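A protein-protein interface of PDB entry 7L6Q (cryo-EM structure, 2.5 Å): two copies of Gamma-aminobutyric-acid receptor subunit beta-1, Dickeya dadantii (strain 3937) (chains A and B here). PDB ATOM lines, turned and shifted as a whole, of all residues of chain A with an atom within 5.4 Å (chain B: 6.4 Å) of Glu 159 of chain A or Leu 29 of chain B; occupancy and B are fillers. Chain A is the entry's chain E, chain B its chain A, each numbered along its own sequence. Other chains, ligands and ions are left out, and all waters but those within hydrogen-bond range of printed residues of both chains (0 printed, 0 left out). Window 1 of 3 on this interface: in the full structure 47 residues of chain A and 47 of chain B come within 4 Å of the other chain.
The backbone carbonyl oxygen (O) of Ile 157 of chain A lies within hydrogen-bond range of the side-chain amide nitrogen (NE2) of Gln 31 of chain B, at 3.3 Å. OH of Tyr 204 of chain A is in hydrogen-bond range of NH2 of Arg 255 of chain B (3.3 Å). ND2 of Asn 200 of chain A sits at hydrogen-bond distance from O of Pro 257 of chain B (3.4 Å).
The side-chain amide oxygen (OD1) of Asn 27 of chain B lies within hydrogen-bond range of the backbone NH (N) of Leu 29 of chain B. OG1 of Thr 28 of chain B sits at hydrogen-bond distance from O of Arg 255 of chain B, 2.8 Å away. The side-chain amide nitrogen of Asn 200 of chain A is in hydrogen-bond range of the backbone carbonyl oxygen of Asp 158 of chain A (3.2 Å). The backbone carbonyl oxygen of Glu 159 of chain A lies within hydrogen-bond range of the backbone NH of Asn 200 of chain A, 3.3 Å away.
Among the printed residues, pairs that only touch across the chains: Glu 159 of chain A with Leu 29 of chain B (3.3 Å), Asp 158 of chain A with Gln 31 of chain B (3.6 Å) and Glu 159 of chain A with Pro 257 of chain B (3.9 Å).
Of chain B, only Leu 29 (3.3 Å) and Pro 257 (3.9 Å) come within 4 Å of Glu 159 of chain A. Of the printed residues of chain A, Leu 29 of chain B touches Glu 159. Of the printed residues of chain B, Asn 200 of chain A touches Pro 257 (3.4 Å). Of the printed residues of chain A, Arg 255 of chain B touches Tyr 204. Printed residues of chain B within 4 Å of Tyr 204 of chain A: Arg 255 (3.3 Å). Of the printed residues of chain B, Ile 157 of chain A touches Gln 31 (3.3 Å). Arg 199 of chain A touches none of the printed residues of chain B. The nearest printed residue of chain A that does not touch Leu 29 of chain B is Tyr 204 of chain A (6.5 Å). The nearest printed residue of chain B that does not touch Tyr 204 of chain A is Leu 256 of chain B (5.5 Å).
Printed residues of chain A that touch a printed residue of chain B: Ile 157, Asp 158, Glu 159, Asn 200 and Tyr 204. Hydrophobic or aromatic side chains of chain A within 4 Å of the printed part of chain B: Tyr 204. Along chain A the printed residues that touch a printed residue of chain B span positions 157 to 204. Of the 10 printed residues of chain B, 4 touch a printed residue of chain A. Printed residues of chain B that touch a printed residue of chain A: Leu 29, Gln 31, Arg 255 and Pro 257. Along chain B the printed residues that touch a printed residue of chain A span positions 29 to 257.
No position is printed for both chains.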
ATOM      1  N   ILE A 157      -1.528 -28.800  16.247  1.00  0.00           N
ATOM      2  CA  ILE A 157      -0.251 -29.328  15.790  1.00  0.00           C
ATOM      3  C   ILE A 157       0.927 -28.570  16.371  1.00  0.00           C
ATOM      4  O   ILE A 157       2.074 -28.846  15.999  1.00  0.00           O
ATOM      5  CB  ILE A 157      -0.163 -29.329  14.253  1.00  0.00           C
ATOM      6  CG1 ILE A 157       0.061 -27.915  13.733  1.00  0.00           C
ATOM      7  CG2 ILE A 157      -1.424 -29.900  13.660  1.00  0.00           C
ATOM      8  CD1 ILE A 157       0.191 -27.843  12.244  1.00  0.00           C
ATOM      9  N   ASP A 158       0.683 -27.624  17.270  1.00  0.00           N
ATOM     10  CA  ASP A 158       1.731 -26.827  17.884  1.00  0.00           C
ATOM     11  C   ASP A 158       1.976 -27.293  19.310  1.00  0.00           C
ATOM     12  O   ASP A 158       1.060 -27.740  20.002  1.00  0.00           O
ATOM     13  CB  ASP A 158       1.372 -25.342  17.882  1.00  0.00           C
ATOM     14  CG  ASP A 158       1.521 -24.709  16.520  1.00  0.00           C
ATOM     15  OD1 ASP A 158       1.892 -25.426  15.568  1.00  0.00           O
ATOM     16  OD2 ASP A 158       1.272 -23.493  16.397  1.00  0.00           O
ATOM     17  N   GLU A 159       3.226 -27.174  19.744  1.00  0.00           N
ATOM     18  CA  GLU A 159       3.608 -27.623  21.071  1.00  0.00           C
ATOM     19  C   GLU A 159       3.083 -26.722  22.176  1.00  0.00           C
ATOM     20  O   GLU A 159       2.794 -27.216  23.268  1.00  0.00           O
ATOM     21  CB  GLU A 159       5.125 -27.714  21.162  1.00  0.00           C
ATOM     22  CG  GLU A 159       5.628 -28.356  22.421  1.00  0.00           C
ATOM     23  CD  GLU A 159       7.132 -28.422  22.458  1.00  0.00           C
ATOM     24  OE1 GLU A 159       7.768 -27.813  21.575  1.00  0.00           O
ATOM     25  OE2 GLU A 159       7.680 -29.081  23.363  1.00  0.00           O
ATOM     26  N   TRP A 160       2.952 -25.423  21.924  1.00  0.00           N
ATOM     27  CA  TRP A 160       2.515 -24.466  22.930  1.00  0.00           C
ATOM     28  C   TRP A 160       1.288 -23.727  22.434  1.00  0.00           C
ATOM     29  O   TRP A 160       1.275 -23.230  21.307  1.00  0.00           O
ATOM     30  CB  TRP A 160       3.618 -23.462  23.254  1.00  0.00           C
ATOM     31  CG  TRP A 160       4.741 -24.046  24.005  1.00  0.00           C
ATOM     32  CD1 TRP A 160       5.903 -24.515  23.494  1.00  0.00           C
ATOM     33  CD2 TRP A 160       4.816 -24.230  25.413  1.00  0.00           C
ATOM     34  NE1 TRP A 160       6.702 -24.985  24.498  1.00  0.00           N
ATOM     35  CE2 TRP A 160       6.053 -24.820  25.690  1.00  0.00           C
ATOM     36  CE3 TRP A 160       3.952 -23.956  26.470  1.00  0.00           C
ATOM     37  CZ2 TRP A 160       6.449 -25.137  26.973  1.00  0.00           C
ATOM     38  CZ3 TRP A 160       4.347 -24.272  27.737  1.00  0.00           C
ATOM     39  CH2 TRP A 160       5.582 -24.855  27.983  1.00  0.00           C
ATOM     40  N   TRP A 161       0.270 -23.647  23.275  1.00  0.00           N
ATOM     41  CA  TRP A 161      -0.914 -22.862  22.977  1.00  0.00           C
ATOM     42  C   TRP A 161      -0.785 -21.508  23.651  1.00  0.00           C
ATOM     43  O   TRP A 161      -0.463 -21.433  24.838  1.00  0.00           O
ATOM     44  CB  TRP A 161      -2.174 -23.567  23.463  1.00  0.00           C
ATOM     45  CG  TRP A 161      -2.359 -24.922  22.897  1.00  0.00           C
ATOM     46  CD1 TRP A 161      -1.800 -25.419  21.767  1.00  0.00           C
ATOM     47  CD2 TRP A 161      -3.156 -25.969  23.445  1.00  0.00           C
ATOM     48  NE1 TRP A 161      -2.204 -26.712  21.570  1.00  0.00           N
ATOM     49  CE2 TRP A 161      -3.037 -27.073  22.592  1.00  0.00           C
ATOM     50  CE3 TRP A 161      -3.958 -26.080  24.580  1.00  0.00           C
ATOM     51  CZ2 TRP A 161      -3.690 -28.266  22.832  1.00  0.00           C
ATOM     52  CZ3 TRP A 161      -4.603 -27.263  24.815  1.00  0.00           C
ATOM     53  CH2 TRP A 161      -4.466 -28.343  23.949  1.00  0.00           C
ATOM     54  N   VAL A 198       0.155 -22.333  27.474  1.00  0.00           N
ATOM     55  CA  VAL A 198      -0.228 -23.583  28.112  1.00  0.00           C
ATOM     56  C   VAL A 198       0.342 -24.717  27.284  1.00  0.00           C
ATOM     57  O   VAL A 198       0.205 -24.718  26.057  1.00  0.00           O
ATOM     58  CB  VAL A 198      -1.752 -23.724  28.231  1.00  0.00           C
ATOM     59  CG1 VAL A 198      -2.098 -25.064  28.812  1.00  0.00           C
ATOM     60  CG2 VAL A 198      -2.309 -22.625  29.087  1.00  0.00           C
ATOM     61  N   ARG A 199       0.983 -25.674  27.941  1.00  0.00           N
ATOM     62  CA  ARG A 199       1.558 -26.791  27.216  1.00  0.00           C
ATOM     63  C   ARG A 199       0.452 -27.652  26.623  1.00  0.00           C
ATOM     64  O   ARG A 199      -0.687 -27.643  27.085  1.00  0.00           O
ATOM     65  CB  ARG A 199       2.446 -27.626  28.129  1.00  0.00           C
ATOM     66  CG  ARG A 199       3.349 -28.582  27.397  1.00  0.00           C
ATOM     67  CD  ARG A 199       4.126 -29.423  28.356  1.00  0.00           C
ATOM     68  NE  ARG A 199       5.055 -28.628  29.138  1.00  0.00           N
ATOM     69  CZ  ARG A 199       6.321 -28.440  28.804  1.00  0.00           C
ATOM     70  NH1 ARG A 199       6.801 -28.992  27.705  1.00  0.00           N
ATOM     71  NH2 ARG A 199       7.109 -27.704  29.567  1.00  0.00           N
ATOM     72  N   ASN A 200       0.799 -28.386  25.573  1.00  0.00           N
ATOM     73  CA  ASN A 200      -0.130 -29.250  24.861  1.00  0.00           C
ATOM     74  C   ASN A 200      -0.116 -30.639  25.483  1.00  0.00           C
ATOM     75  O   ASN A 200       0.768 -31.444  25.175  1.00  0.00           O
ATOM     76  CB  ASN A 200       0.249 -29.309  23.382  1.00  0.00           C
ATOM     77  CG  ASN A 200      -0.725 -30.110  22.561  1.00  0.00           C
ATOM     78  OD1 ASN A 200      -1.776 -30.513  23.044  1.00  0.00           O
ATOM     79  ND2 ASN A 200      -0.384 -30.342  21.304  1.00  0.00           N
ATOM     80  N   TYR A 204       1.762 -36.437  26.247  1.00  0.00           N
ATOM     81  CA  TYR A 204       2.106 -36.860  27.594  1.00  0.00           C
ATOM     82  C   TYR A 204       0.926 -37.438  28.349  1.00  0.00           C
ATOM     83  O   TYR A 204       1.123 -38.033  29.411  1.00  0.00           O
ATOM     84  CB  TYR A 204       2.687 -35.686  28.375  1.00  0.00           C
ATOM     85  CG  TYR A 204       3.824 -35.026  27.659  1.00  0.00           C
ATOM     86  CD1 TYR A 204       5.058 -35.632  27.585  1.00  0.00           C
ATOM     87  CD2 TYR A 204       3.659 -33.804  27.044  1.00  0.00           C
ATOM     88  CE1 TYR A 204       6.096 -35.039  26.928  1.00  0.00           C
ATOM     89  CE2 TYR A 204       4.693 -33.203  26.383  1.00  0.00           C
ATOM     90  CZ  TYR A 204       5.910 -33.825  26.329  1.00  0.00           C
ATOM     91  OH  TYR A 204       6.953 -33.230  25.668  1.00  0.00           O
ATOM     92  N   ASN B  27      13.650 -30.801  11.393  1.00  0.00           N
ATOM     93  CA  ASN B  27      13.507 -30.842  12.842  1.00  0.00           C
ATOM     94  C   ASN B  27      12.020 -30.786  13.160  1.00  0.00           C
ATOM     95  O   ASN B  27      11.358 -29.783  12.885  1.00  0.00           O
ATOM     96  CB  ASN B  27      14.258 -29.681  13.486  1.00  0.00           C
ATOM     97  CG  ASN B  27      14.349 -29.806  14.982  1.00  0.00           C
ATOM     98  OD1 ASN B  27      13.590 -30.540  15.606  1.00  0.00           O
ATOM     99  ND2 ASN B  27      15.283 -29.080  15.574  1.00  0.00           N
ATOM    100  N   THR B  28      11.497 -31.861  13.745  1.00  0.00           N
ATOM    101  CA  THR B  28      10.054 -31.991  13.893  1.00  0.00           C
ATOM    102  C   THR B  28       9.494 -31.142  15.023  1.00  0.00           C
ATOM    103  O   THR B  28       8.357 -30.674  14.927  1.00  0.00           O
ATOM    104  CB  THR B  28       9.692 -33.449  14.116  1.00  0.00           C
ATOM    105  OG1 THR B  28      10.517 -33.979  15.156  1.00  0.00           O
ATOM    106  CG2 THR B  28       9.925 -34.234  12.855  1.00  0.00           C
ATOM    107  N   LEU B  29      10.250 -30.945  16.101  1.00  0.00           N
ATOM    108  CA  LEU B  29       9.734 -30.147  17.207  1.00  0.00           C
ATOM    109  C   LEU B  29       9.685 -28.670  16.850  1.00  0.00           C
ATOM    110  O   LEU B  29       8.692 -27.992  17.128  1.00  0.00           O
ATOM    111  CB  LEU B  29      10.582 -30.364  18.454  1.00  0.00           C
ATOM    112  CG  LEU B  29       9.880 -31.119  19.574  1.00  0.00           C
ATOM    113  CD1 LEU B  29      10.724 -31.106  20.829  1.00  0.00           C
ATOM    114  CD2 LEU B  29       8.525 -30.514  19.836  1.00  0.00           C
ATOM    115  N   GLU B  30      10.748 -28.153  16.240  1.00  0.00           N
ATOM    116  CA  GLU B  30      10.794 -26.755  15.843  1.00  0.00           C
ATOM    117  C   GLU B  30      10.080 -26.489  14.531  1.00  0.00           C
ATOM    118  O   GLU B  30       9.844 -25.323  14.204  1.00  0.00           O
ATOM    119  CB  GLU B  30      12.241 -26.293  15.720  1.00  0.00           C
ATOM    120  CG  GLU B  30      13.081 -26.573  16.934  1.00  0.00           C
ATOM    121  CD  GLU B  30      14.512 -26.137  16.747  1.00  0.00           C
ATOM    122  OE1 GLU B  30      14.839 -25.644  15.648  1.00  0.00           O
ATOM    123  OE2 GLU B  30      15.311 -26.284  17.695  1.00  0.00           O
ATOM    124  N   GLN B  31       9.737 -27.531  13.781  1.00  0.00           N
ATOM    125  CA  GLN B  31       9.108 -27.395  12.473  1.00  0.00           C
ATOM    126  C   GLN B  31       9.972 -26.559  11.533  1.00  0.00           C
ATOM    127  O   GLN B  31       9.496 -25.651  10.855  1.00  0.00           O
ATOM    128  CB  GLN B  31       7.703 -26.812  12.602  1.00  0.00           C
ATOM    129  CG  GLN B  31       6.806 -27.634  13.490  1.00  0.00           C
ATOM    130  CD  GLN B  31       5.424 -27.058  13.614  1.00  0.00           C
ATOM    131  OE1 GLN B  31       5.017 -26.223  12.819  1.00  0.00           O
ATOM    132  NE2 GLN B  31       4.692 -27.501  14.620  1.00  0.00           N
ATOM    133  N   THR B  32      11.261 -26.876  11.501  1.00  0.00           N
ATOM    134  CA  THR B  32      12.214 -26.206  10.634  1.00  0.00           C
ATOM    135  C   THR B  32      12.940 -27.222   9.768  1.00  0.00           C
ATOM    136  O   THR B  32      12.960 -28.420  10.049  1.00  0.00           O
ATOM    137  CB  THR B  32      13.239 -25.397  11.434  1.00  0.00           C
ATOM    138  OG1 THR B  32      14.136 -26.289  12.100  1.00  0.00           O
ATOM    139  CG2 THR B  32      12.552 -24.526  12.456  1.00  0.00           C
ATOM    140  N   PHE B 116       2.804 -33.622  11.312  1.00  0.00           N
ATOM    141  CA  PHE B 116       3.318 -34.984  11.238  1.00  0.00           C
ATOM    142  C   PHE B 116       2.353 -36.013  11.813  1.00  0.00           C
ATOM    143  O   PHE B 116       2.791 -37.058  12.300  1.00  0.00           O
ATOM    144  CB  PHE B 116       4.655 -35.088  11.967  1.00  0.00           C
ATOM    145  CG  PHE B 116       5.717 -34.195  11.427  1.00  0.00           C
ATOM    146  CD1 PHE B 116       6.393 -34.524  10.278  1.00  0.00           C
ATOM    147  CD2 PHE B 116       6.061 -33.038  12.085  1.00  0.00           C
ATOM    148  CE1 PHE B 116       7.374 -33.710   9.786  1.00  0.00           C
ATOM    149  CE2 PHE B 116       7.045 -32.223  11.596  1.00  0.00           C
ATOM    150  CZ  PHE B 116       7.700 -32.560  10.446  1.00  0.00           C
ATOM    151  N   ARG B 255      10.710 -36.547  17.906  1.00  0.00           N
ATOM    152  CA  ARG B 255       9.854 -36.035  18.964  1.00  0.00           C
ATOM    153  C   ARG B 255       8.733 -35.190  18.380  1.00  0.00           C
ATOM    154  O   ARG B 255       8.943 -34.403  17.456  1.00  0.00           O
ATOM    155  CB  ARG B 255      10.673 -35.213  19.953  1.00  0.00           C
ATOM    156  CG  ARG B 255      11.653 -36.024  20.778  1.00  0.00           C
ATOM    157  CD  ARG B 255      10.934 -37.036  21.646  1.00  0.00           C
ATOM    158  NE  ARG B 255       9.653 -36.524  22.122  1.00  0.00           N
ATOM    159  CZ  ARG B 255       9.510 -35.699  23.152  1.00  0.00           C
ATOM    160  NH1 ARG B 255      10.572 -35.285  23.828  1.00  0.00           N
ATOM    161  NH2 ARG B 255       8.302 -35.285  23.506  1.00  0.00           N
ATOM    162  N   LEU B 256       7.536 -35.357  18.921  1.00  0.00           N
ATOM    163  CA  LEU B 256       6.354 -34.662  18.446  1.00  0.00           C
ATOM    164  C   LEU B 256       5.478 -34.308  19.633  1.00  0.00           C
ATOM    165  O   LEU B 256       5.553 -34.956  20.683  1.00  0.00           O
ATOM    166  CB  LEU B 256       5.568 -35.522  17.451  1.00  0.00           C
ATOM    167  CG  LEU B 256       6.247 -35.750  16.111  1.00  0.00           C
ATOM    168  CD1 LEU B 256       5.458 -36.721  15.290  1.00  0.00           C
ATOM    169  CD2 LEU B 256       6.366 -34.439  15.392  1.00  0.00           C
ATOM    170  N   PRO B 257       4.642 -33.281  19.505  1.00  0.00           N
ATOM    171  CA  PRO B 257       3.690 -32.941  20.569  1.00  0.00           C
ATOM    172  C   PRO B 257       2.341 -33.636  20.470  1.00  0.00           C
ATOM    173  O   PRO B 257       1.417 -33.235  21.180  1.00  0.00           O
ATOM    174  CB  PRO B 257       3.522 -31.434  20.373  1.00  0.00           C
ATOM    175  CG  PRO B 257       3.647 -31.261  18.924  1.00  0.00           C
ATOM    176  CD  PRO B 257       4.669 -32.252  18.456  1.00  0.00           C
